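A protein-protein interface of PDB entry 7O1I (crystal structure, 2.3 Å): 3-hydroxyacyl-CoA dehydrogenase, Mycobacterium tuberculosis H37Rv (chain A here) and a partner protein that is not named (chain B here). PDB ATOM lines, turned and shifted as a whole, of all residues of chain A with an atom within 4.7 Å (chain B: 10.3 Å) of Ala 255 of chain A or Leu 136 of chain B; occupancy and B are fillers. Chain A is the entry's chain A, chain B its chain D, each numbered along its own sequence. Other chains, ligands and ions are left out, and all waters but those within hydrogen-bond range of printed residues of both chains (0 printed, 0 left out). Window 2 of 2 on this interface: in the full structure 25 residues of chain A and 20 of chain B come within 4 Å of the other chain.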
ATOM      1  N   PRO A 249     -32.218  -1.460  -8.948  1.00  0.00           N
ATOM      2  CA  PRO A 249     -30.854  -1.469  -9.510  1.00  0.00           C
ATOM      3  C   PRO A 249     -29.923  -2.501  -8.885  1.00  0.00           C
ATOM      4  O   PRO A 249     -28.865  -2.776  -9.467  1.00  0.00           O
ATOM      5  CB  PRO A 249     -30.358  -0.042  -9.246  1.00  0.00           C
ATOM      6  CG  PRO A 249     -31.601   0.777  -9.265  1.00  0.00           C
ATOM      7  CD  PRO A 249     -32.667  -0.088  -8.643  1.00  0.00           C
ATOM      8  N   SER A 251     -30.999  -5.688  -8.209  1.00  0.00           N
ATOM      9  CA  SER A 251     -31.396  -6.998  -8.703  1.00  0.00           C
ATOM     10  C   SER A 251     -30.490  -7.420  -9.858  1.00  0.00           C
ATOM     11  O   SER A 251     -30.129  -6.590 -10.698  1.00  0.00           O
ATOM     12  CB  SER A 251     -32.853  -6.981  -9.166  1.00  0.00           C
ATOM     13  OG  SER A 251     -33.715  -6.551  -8.125  1.00  0.00           O
ATOM     14  N   PRO A 252     -30.113  -8.700  -9.933  1.00  0.00           N
ATOM     15  CA  PRO A 252     -29.202  -9.126 -11.007  1.00  0.00           C
ATOM     16  C   PRO A 252     -29.820  -9.040 -12.391  1.00  0.00           C
ATOM     17  O   PRO A 252     -29.083  -8.909 -13.377  1.00  0.00           O
ATOM     18  CB  PRO A 252     -28.865 -10.573 -10.626  1.00  0.00           C
ATOM     19  CG  PRO A 252     -30.045 -11.029  -9.832  1.00  0.00           C
ATOM     20  CD  PRO A 252     -30.515  -9.821  -9.066  1.00  0.00           C
ATOM     21  N   GLY A 253     -31.148  -9.111 -12.498  1.00  0.00           N
ATOM     22  CA  GLY A 253     -31.777  -9.012 -13.806  1.00  0.00           C
ATOM     23  C   GLY A 253     -31.739  -7.601 -14.363  1.00  0.00           C
ATOM     24  O   GLY A 253     -31.383  -7.389 -15.526  1.00  0.00           O
ATOM     25  N   LEU A 254     -32.105  -6.614 -13.540  1.00  0.00           N
ATOM     26  CA  LEU A 254     -32.112  -5.231 -14.007  1.00  0.00           C
ATOM     27  C   LEU A 254     -30.697  -4.683 -14.145  1.00  0.00           C
ATOM     28  O   LEU A 254     -30.392  -3.973 -15.112  1.00  0.00           O
ATOM     29  CB  LEU A 254     -32.934  -4.355 -13.061  1.00  0.00           C
ATOM     30  CG  LEU A 254     -32.959  -2.863 -13.400  1.00  0.00           C
ATOM     31  CD1 LEU A 254     -33.480  -2.643 -14.809  1.00  0.00           C
ATOM     32  CD2 LEU A 254     -33.793  -2.085 -12.398  1.00  0.00           C
ATOM     33  N   ALA A 255     -29.818  -5.001 -13.191  1.00  0.00           N
ATOM     34  CA  ALA A 255     -28.447  -4.507 -13.245  1.00  0.00           C
ATOM     35  C   ALA A 255     -27.683  -5.042 -14.450  1.00  0.00           C
ATOM     36  O   ALA A 255     -26.668  -4.452 -14.835  1.00  0.00           O
ATOM     37  CB  ALA A 255     -27.705  -4.866 -11.957  1.00  0.00           C
ATOM     38  N   ALA A 256     -28.144  -6.141 -15.052  1.00  0.00           N
ATOM     39  CA  ALA A 256     -27.466  -6.671 -16.229  1.00  0.00           C
ATOM     40  C   ALA A 256     -27.687  -5.792 -17.453  1.00  0.00           C
ATOM     41  O   ALA A 256     -26.833  -5.750 -18.346  1.00  0.00           O
ATOM     42  CB  ALA A 256     -27.933  -8.100 -16.508  1.00  0.00           C
ATOM     43  N   ILE A 257     -28.817  -5.088 -17.517  1.00  0.00           N
ATOM     44  CA  ILE A 257     -29.119  -4.202 -18.638  1.00  0.00           C
ATOM     45  C   ILE A 257     -29.078  -2.735 -18.253  1.00  0.00           C
ATOM     46  O   ILE A 257     -29.158  -1.875 -19.148  1.00  0.00           O
ATOM     47  CB  ILE A 257     -30.483  -4.538 -19.274  1.00  0.00           C
ATOM     48  CG1 ILE A 257     -31.603  -4.402 -18.241  1.00  0.00           C
ATOM     49  CG2 ILE A 257     -30.464  -5.940 -19.873  1.00  0.00           C
ATOM     50  CD1 ILE A 257     -32.980  -4.673 -18.800  1.00  0.00           C
ATOM     51  N   LEU A 258     -28.961  -2.420 -16.965  1.00  0.00           N
ATOM     52  CA  LEU A 258     -28.917  -1.026 -16.531  1.00  0.00           C
ATOM     53  C   LEU A 258     -27.798  -0.210 -17.174  1.00  0.00           C
ATOM     54  O   LEU A 258     -28.029   0.981 -17.447  1.00  0.00           O
ATOM     55  CB  LEU A 258     -28.815  -0.982 -15.002  1.00  0.00           C
ATOM     56  CG  LEU A 258     -29.038   0.356 -14.300  1.00  0.00           C
ATOM     57  CD1 LEU A 258     -30.434   0.885 -14.589  1.00  0.00           C
ATOM     58  CD2 LEU A 258     -28.821   0.187 -12.807  1.00  0.00           C
ATOM     59  N   PRO A 259     -26.596  -0.744 -17.429  1.00  0.00           N
ATOM     60  CA  PRO A 259     -25.581   0.069 -18.121  1.00  0.00           C
ATOM     61  C   PRO A 259     -25.973   0.498 -19.525  1.00  0.00           C
ATOM     62  O   PRO A 259     -25.375   1.443 -20.051  1.00  0.00           O
ATOM     63  CB  PRO A 259     -24.352  -0.849 -18.142  1.00  0.00           C
ATOM     64  CG  PRO A 259     -24.534  -1.732 -16.976  1.00  0.00           C
ATOM     65  CD  PRO A 259     -26.007  -1.989 -16.899  1.00  0.00           C
ATOM     66  N   VAL A 285     -33.526   6.142 -11.383  1.00  0.00           N
ATOM     67  CA  VAL A 285     -32.708   5.031 -10.905  1.00  0.00           C
ATOM     68  C   VAL A 285     -32.259   5.270  -9.468  1.00  0.00           C
ATOM     69  O   VAL A 285     -32.316   4.364  -8.628  1.00  0.00           O
ATOM     70  CB  VAL A 285     -31.512   4.808 -11.846  1.00  0.00           C
ATOM     71  CG1 VAL A 285     -30.579   3.749 -11.280  1.00  0.00           C
ATOM     72  CG2 VAL A 285     -31.999   4.408 -13.227  1.00  0.00           C
ATOM     73  N   MET B 127     -18.023 -11.400 -13.793  1.00  0.00           N
ATOM     74  CA  MET B 127     -17.638 -10.010 -14.016  1.00  0.00           C
ATOM     75  C   MET B 127     -18.770  -9.066 -13.633  1.00  0.00           C
ATOM     76  O   MET B 127     -19.946  -9.344 -13.882  1.00  0.00           O
ATOM     77  CB  MET B 127     -17.266  -9.789 -15.481  1.00  0.00           C
ATOM     78  CG  MET B 127     -15.937 -10.378 -15.900  1.00  0.00           C
ATOM     79  SD  MET B 127     -15.649 -10.191 -17.672  1.00  0.00           S
ATOM     80  CE  MET B 127     -16.054  -8.462 -17.896  1.00  0.00           C
ATOM     81  N   GLY B 128     -18.405  -7.933 -13.037  1.00  0.00           N
ATOM     82  CA  GLY B 128     -19.394  -6.944 -12.661  1.00  0.00           C
ATOM     83  C   GLY B 128     -20.309  -7.358 -11.533  1.00  0.00           C
ATOM     84  O   GLY B 128     -21.365  -6.747 -11.352  1.00  0.00           O
ATOM     85  N   SER B 129     -19.936  -8.387 -10.768  1.00  0.00           N
ATOM     86  CA  SER B 129     -20.742  -8.784  -9.619  1.00  0.00           C
ATOM     87  C   SER B 129     -20.728  -7.721  -8.528  1.00  0.00           C
ATOM     88  O   SER B 129     -21.668  -7.641  -7.731  1.00  0.00           O
ATOM     89  CB  SER B 129     -20.244 -10.117  -9.058  1.00  0.00           C
ATOM     90  OG  SER B 129     -20.376 -11.158 -10.008  1.00  0.00           O
ATOM     91  N   ASP B 130     -19.677  -6.904  -8.476  1.00  0.00           N
ATOM     92  CA  ASP B 130     -19.550  -5.849  -7.478  1.00  0.00           C
ATOM     93  C   ASP B 130     -20.320  -4.587  -7.840  1.00  0.00           C
ATOM     94  O   ASP B 130     -20.314  -3.634  -7.053  1.00  0.00           O
ATOM     95  CB  ASP B 130     -18.073  -5.501  -7.270  1.00  0.00           C
ATOM     96  CG  ASP B 130     -17.369  -5.151  -8.568  1.00  0.00           C
ATOM     97  OD1 ASP B 130     -17.764  -5.690  -9.625  1.00  0.00           O
ATOM     98  OD2 ASP B 130     -16.418  -4.340  -8.535  1.00  0.00           O
ATOM     99  N   GLY B 131     -20.977  -4.553  -8.996  1.00  0.00           N
ATOM    100  CA  GLY B 131     -21.650  -3.338  -9.410  1.00  0.00           C
ATOM    101  C   GLY B 131     -20.657  -2.269  -9.837  1.00  0.00           C
ATOM    102  O   GLY B 131     -19.592  -2.549 -10.394  1.00  0.00           O
ATOM    103  N   GLY B 132     -21.014  -1.018  -9.562  1.00  0.00           N
ATOM    104  CA  GLY B 132     -20.169   0.102  -9.928  1.00  0.00           C
ATOM    105  C   GLY B 132     -20.955   1.301 -10.414  1.00  0.00           C
ATOM    106  O   GLY B 132     -21.983   1.149 -11.082  1.00  0.00           O
ATOM    107  N   ALA B 133     -20.479   2.504 -10.089  1.00  0.00           N
ATOM    108  CA  ALA B 133     -21.205   3.708 -10.479  1.00  0.00           C
ATOM    109  C   ALA B 133     -21.035   4.005 -11.965  1.00  0.00           C
ATOM    110  O   ALA B 133     -21.967   4.491 -12.616  1.00  0.00           O
ATOM    111  CB  ALA B 133     -20.748   4.896  -9.634  1.00  0.00           C
ATOM    112  N   MET B 134     -19.852   3.717 -12.518  1.00  0.00           N
ATOM    113  CA  MET B 134     -19.600   3.990 -13.930  1.00  0.00           C
ATOM    114  C   MET B 134     -20.592   3.277 -14.837  1.00  0.00           C
ATOM    115  O   MET B 134     -20.941   3.794 -15.904  1.00  0.00           O
ATOM    116  CB  MET B 134     -18.178   3.574 -14.303  1.00  0.00           C
ATOM    117  CG  MET B 134     -17.100   4.527 -13.848  1.00  0.00           C
ATOM    118  SD  MET B 134     -15.475   3.809 -14.136  1.00  0.00           S
ATOM    119  CE  MET B 134     -14.436   5.239 -13.895  1.00  0.00           C
ATOM    120  N   GLY B 135     -21.052   2.096 -14.437  1.00  0.00           N
ATOM    121  CA  GLY B 135     -21.967   1.336 -15.260  1.00  0.00           C
ATOM    122  C   GLY B 135     -23.412   1.435 -14.820  1.00  0.00           C
ATOM    123  O   GLY B 135     -24.312   1.509 -15.660  1.00  0.00           O
ATOM    124  N   LEU B 136     -23.653   1.452 -13.508  1.00  0.00           N
ATOM    125  CA  LEU B 136     -25.014   1.362 -12.994  1.00  0.00           C
ATOM    126  C   LEU B 136     -25.619   2.702 -12.590  1.00  0.00           C
ATOM    127  O   LEU B 136     -26.845   2.788 -12.466  1.00  0.00           O
ATOM    128  CB  LEU B 136     -25.060   0.401 -11.800  1.00  0.00           C
ATOM    129  CG  LEU B 136     -24.639  -1.036 -12.125  1.00  0.00           C
ATOM    130  CD1 LEU B 136     -24.721  -1.923 -10.894  1.00  0.00           C
ATOM    131  CD2 LEU B 136     -25.492  -1.599 -13.250  1.00  0.00           C
ATOM    132  N   ASP B 137     -24.810   3.744 -12.382  1.00  0.00           N
ATOM    133  CA  ASP B 137     -25.343   5.059 -12.042  1.00  0.00           C
ATOM    134  C   ASP B 137     -25.510   5.876 -13.316  1.00  0.00           C
ATOM    135  O   ASP B 137     -24.502   6.218 -13.954  1.00  0.00           O
ATOM    136  CB  ASP B 137     -24.427   5.781 -11.062  1.00  0.00           C
ATOM    137  CG  ASP B 137     -24.938   7.166 -10.701  1.00  0.00           C
ATOM    138  OD1 ASP B 137     -26.072   7.265 -10.189  1.00  0.00           O
ATOM    139  OD2 ASP B 137     -24.208   8.155 -10.928  1.00  0.00           O
ATOM    140  N   PRO B 138     -26.740   6.218 -13.719  1.00  0.00           N
ATOM    141  CA  PRO B 138     -26.920   6.896 -15.018  1.00  0.00           C
ATOM    142  C   PRO B 138     -26.162   8.206 -15.146  1.00  0.00           C
ATOM    143  O   PRO B 138     -25.501   8.433 -16.167  1.00  0.00           O
ATOM    144  CB  PRO B 138     -28.439   7.108 -15.087  1.00  0.00           C
ATOM    145  CG  PRO B 138     -29.008   6.068 -14.197  1.00  0.00           C
ATOM    146  CD  PRO B 138     -28.025   5.905 -13.075  1.00  0.00           C
ATOM    147  N   ALA B 139     -26.243   9.081 -14.140  1.00  0.00           N
ATOM    148  CA  ALA B 139     -25.552  10.365 -14.220  1.00  0.00           C
ATOM    149  C   ALA B 139     -24.053  10.177 -14.421  1.00  0.00           C
ATOM    150  O   ALA B 139     -23.424  10.918 -15.185  1.00  0.00           O
ATOM    151  CB  ALA B 139     -25.829  11.193 -12.966  1.00  0.00           C
ATOM    152  N   THR B 140     -23.463   9.185 -13.751  1.00  0.00           N
ATOM    153  CA  THR B 140     -22.043   8.915 -13.953  1.00  0.00           C
ATOM    154  C   THR B 140     -21.798   8.259 -15.305  1.00  0.00           C
ATOM    155  O   THR B 140     -20.834   8.598 -16.002  1.00  0.00           O
ATOM    156  CB  THR B 140     -21.507   8.035 -12.826  1.00  0.00           C
ATOM    157  OG1 THR B 140     -21.857   8.608 -11.562  1.00  0.00           O
ATOM    158  CG2 THR B 140     -19.992   7.917 -12.920  1.00  0.00           C
ATOM    159  N   ASN B 141     -22.663   7.320 -15.692  1.00  0.00           N
ATOM    160  CA  ASN B 141     -22.516   6.644 -16.978  1.00  0.00           C
ATOM    161  C   ASN B 141     -22.704   7.622 -18.132  1.00  0.00           C
ATOM    162  O   ASN B 141     -21.900   7.657 -19.071  1.00  0.00           O
ATOM    163  CB  ASN B 141     -23.522   5.492 -17.064  1.00  0.00           C
ATOM    164  CG  ASN B 141     -23.304   4.600 -18.276  1.00  0.00           C
ATOM    165  OD1 ASN B 141     -23.164   5.074 -19.403  1.00  0.00           O
ATOM    166  ND2 ASN B 141     -23.287   3.292 -18.044  1.00  0.00           N
ATOM    167  N   TYR B 142     -23.764   8.432 -18.072  1.00  0.00           N
ATOM    168  CA  TYR B 142     -24.077   9.342 -19.168  1.00  0.00           C
ATOM    169  C   TYR B 142     -22.994  10.396 -19.359  1.00  0.00           C
ATOM    170  O   TYR B 142     -22.751  10.836 -20.488  1.00  0.00           O
ATOM    171  CB  TYR B 142     -25.431  10.008 -18.911  1.00  0.00           C
ATOM    172  CG  TYR B 142     -25.999  10.798 -20.070  1.00  0.00           C
ATOM    173  CD1 TYR B 142     -25.646  12.126 -20.275  1.00  0.00           C
ATOM    174  CD2 TYR B 142     -26.913  10.221 -20.943  1.00  0.00           C
ATOM    175  CE1 TYR B 142     -26.176  12.854 -21.330  1.00  0.00           C
ATOM    176  CE2 TYR B 142     -27.449  10.942 -21.999  1.00  0.00           C
ATOM    177  CZ  TYR B 142     -27.077  12.256 -22.187  1.00  0.00           C
ATOM    178  OH  TYR B 142     -27.608  12.972 -23.237  1.00  0.00           O
ATOM    179  N   VAL B 144     -19.504  10.317 -18.324  1.00  0.00           N
ATOM    180  CA  VAL B 144     -18.202   9.805 -18.752  1.00  0.00           C
ATOM    181  C   VAL B 144     -18.268   9.049 -20.067  1.00  0.00           C
ATOM    182  O   VAL B 144     -17.219   8.639 -20.583  1.00  0.00           O
ATOM    183  CB  VAL B 144     -17.578   8.877 -17.690  1.00  0.00           C
ATOM    184  CG1 VAL B 144     -17.576   9.554 -16.327  1.00  0.00           C
ATOM    185  CG2 VAL B 144     -18.315   7.546 -17.648  1.00  0.00           C
ATOM    186  N   PHE B 146     -19.665   5.910 -20.910  1.00  0.00           N
ATOM    187  CA  PHE B 146     -19.190   4.559 -20.656  1.00  0.00           C
ATOM    188  C   PHE B 146     -19.547   3.641 -21.817  1.00  0.00           C
ATOM    189  O   PHE B 146     -20.709   3.566 -22.228  1.00  0.00           O
ATOM    190  CB  PHE B 146     -19.786   4.023 -19.354  1.00  0.00           C
ATOM    191  CG  PHE B 146     -19.702   2.528 -19.216  1.00  0.00           C
ATOM    192  CD1 PHE B 146     -18.523   1.918 -18.814  1.00  0.00           C
ATOM    193  CD2 PHE B 146     -20.805   1.730 -19.482  1.00  0.00           C
ATOM    194  CE1 PHE B 146     -18.445   0.541 -18.685  1.00  0.00           C
ATOM    195  CE2 PHE B 146     -20.733   0.353 -19.357  1.00  0.00           C
ATOM    196  CZ  PHE B 146     -19.552  -0.241 -18.956  1.00  0.00           C
ATOM    197  N   LEU B 228     -24.167  -6.905 -28.409  1.00  0.00           N
ATOM    198  CA  LEU B 228     -24.018  -5.998 -27.276  1.00  0.00           C
ATOM    199  C   LEU B 228     -24.051  -4.543 -27.728  1.00  0.00           C
ATOM    200  O   LEU B 228     -24.635  -3.688 -27.051  1.00  0.00           O
ATOM    201  CB  LEU B 228     -22.716  -6.304 -26.534  1.00  0.00           C
ATOM    202  CG  LEU B 228     -22.237  -5.290 -25.494  1.00  0.00           C
ATOM    203  CD1 LEU B 228     -23.220  -5.188 -24.336  1.00  0.00           C
ATOM    204  CD2 LEU B 228     -20.847  -5.656 -24.998  1.00  0.00           C
ATOM    205  N   PHE B 234     -24.006   1.178 -27.517  1.00  0.00           N
ATOM    206  CA  PHE B 234     -22.662   1.633 -27.182  1.00  0.00           C
ATOM    207  C   PHE B 234     -21.853   2.020 -28.413  1.00  0.00           C
ATOM    208  O   PHE B 234     -20.874   2.763 -28.285  1.00  0.00           O
ATOM    209  CB  PHE B 234     -21.922   0.554 -26.388  1.00  0.00           C
ATOM    210  CG  PHE B 234     -22.613   0.154 -25.113  1.00  0.00           C
ATOM    211  CD1 PHE B 234     -22.589   0.986 -24.005  1.00  0.00           C
ATOM    212  CD2 PHE B 234     -23.281  -1.056 -25.021  1.00  0.00           C
ATOM    213  CE1 PHE B 234     -23.223   0.619 -22.829  1.00  0.00           C
ATOM    214  CE2 PHE B 234     -23.916  -1.428 -23.849  1.00  0.00           C
ATOM    215  CZ  PHE B 234     -23.887  -0.589 -22.752  1.00  0.00           C
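The backbone carbonyl oxygen (O) of Met 134 of chain B is in hydrogen-bond range of the side-chain amide nitrogen (ND2) of Asn 141 of chain B (3.2 Å). O of Gly 135 of chain B is in hydrogen-bond range of ND2 of Asn 141 of chain B, 3.1 Å away. O of Asn 141 of chain B sits at hydrogen-bond distance from N of Phe 146 of chain B (3.4 Å).
Of chain B, only Leu 136 (3.5 Å) comes within 4 Å of Ala 255 of chain A. Of chain A, only Ala 255, Leu 258 and Pro 259 come within 4 Å of Leu 136 of chain B. No residue of chain B comes within 4 Å of Gly 253 of chain A. No residue of chain B comes within 4 Å of Leu 254 of chain A. No residue of chain B comes within 4 Å of Ala 256 of chain A. Leu 258 of chain A touches one residue of chain B. Printed residues of chain B within 4 Å of Pro 259 of chain A: Gly 135, Leu 136, Asn 141 and Phe 234. Of the printed residues of chain B, Val 285 of chain A touches Pro 138 (3.6 Å). Of the printed residues of chain A, Phe 234 of chain B touches Pro 259 (3.6 Å). Of the printed residues of chain A, Asn 141 of chain B touches Pro 259. Of the printed residues of chain A, Pro 138 of chain B touches Val 285 (3.6 Å). Asp 130 of chain B touches none of the printed residues of chain A. The nearest residue of chain B that does not touch Ala 255 of chain A is Gly 135 of chain B (6.5 Å).
Printed residues of chain A that touch a printed residue of chain B: Ala 255, Leu 258, Pro 259 and Val 285. Hydrophobic or aromatic side chains of chain A that line the printed part of chain B: Leu 258, Pro 259 and Val 285. Of the 20 printed residues of chain B, 5 touch a printed residue of chain A. Printed residues of chain B that touch a printed residue of chain A: Gly 135, Leu 136, Pro 138, Asn 141 and Phe 234. Among the printed residues, 7 pairs touch across the chains. Among the printed residues, no Asp or Glu carboxylate lies within 4 Å of a Lys or Arg side-chain nitrogen of the other chain.
The backbone carbonyl oxygen (O) of Pro 259 of chain A lies within hydrogen-bond range of the side-chain amide nitrogen (ND2) of Asn 141 of chain B, 3.4 Å away.
Among the printed residues, pairs that only touch across the chains: Pro 259 of chain A with Gly 135 of chain B, Leu 258 of chain A with Leu 136 of chain B, Ala 255 of chain A with Leu 136 of chain B, Val 285 of chain A with Pro 138 of chain B, Pro 259 of chain A with Phe 234 of chain B and Pro 259 of chain A with Leu 136 of chain B.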
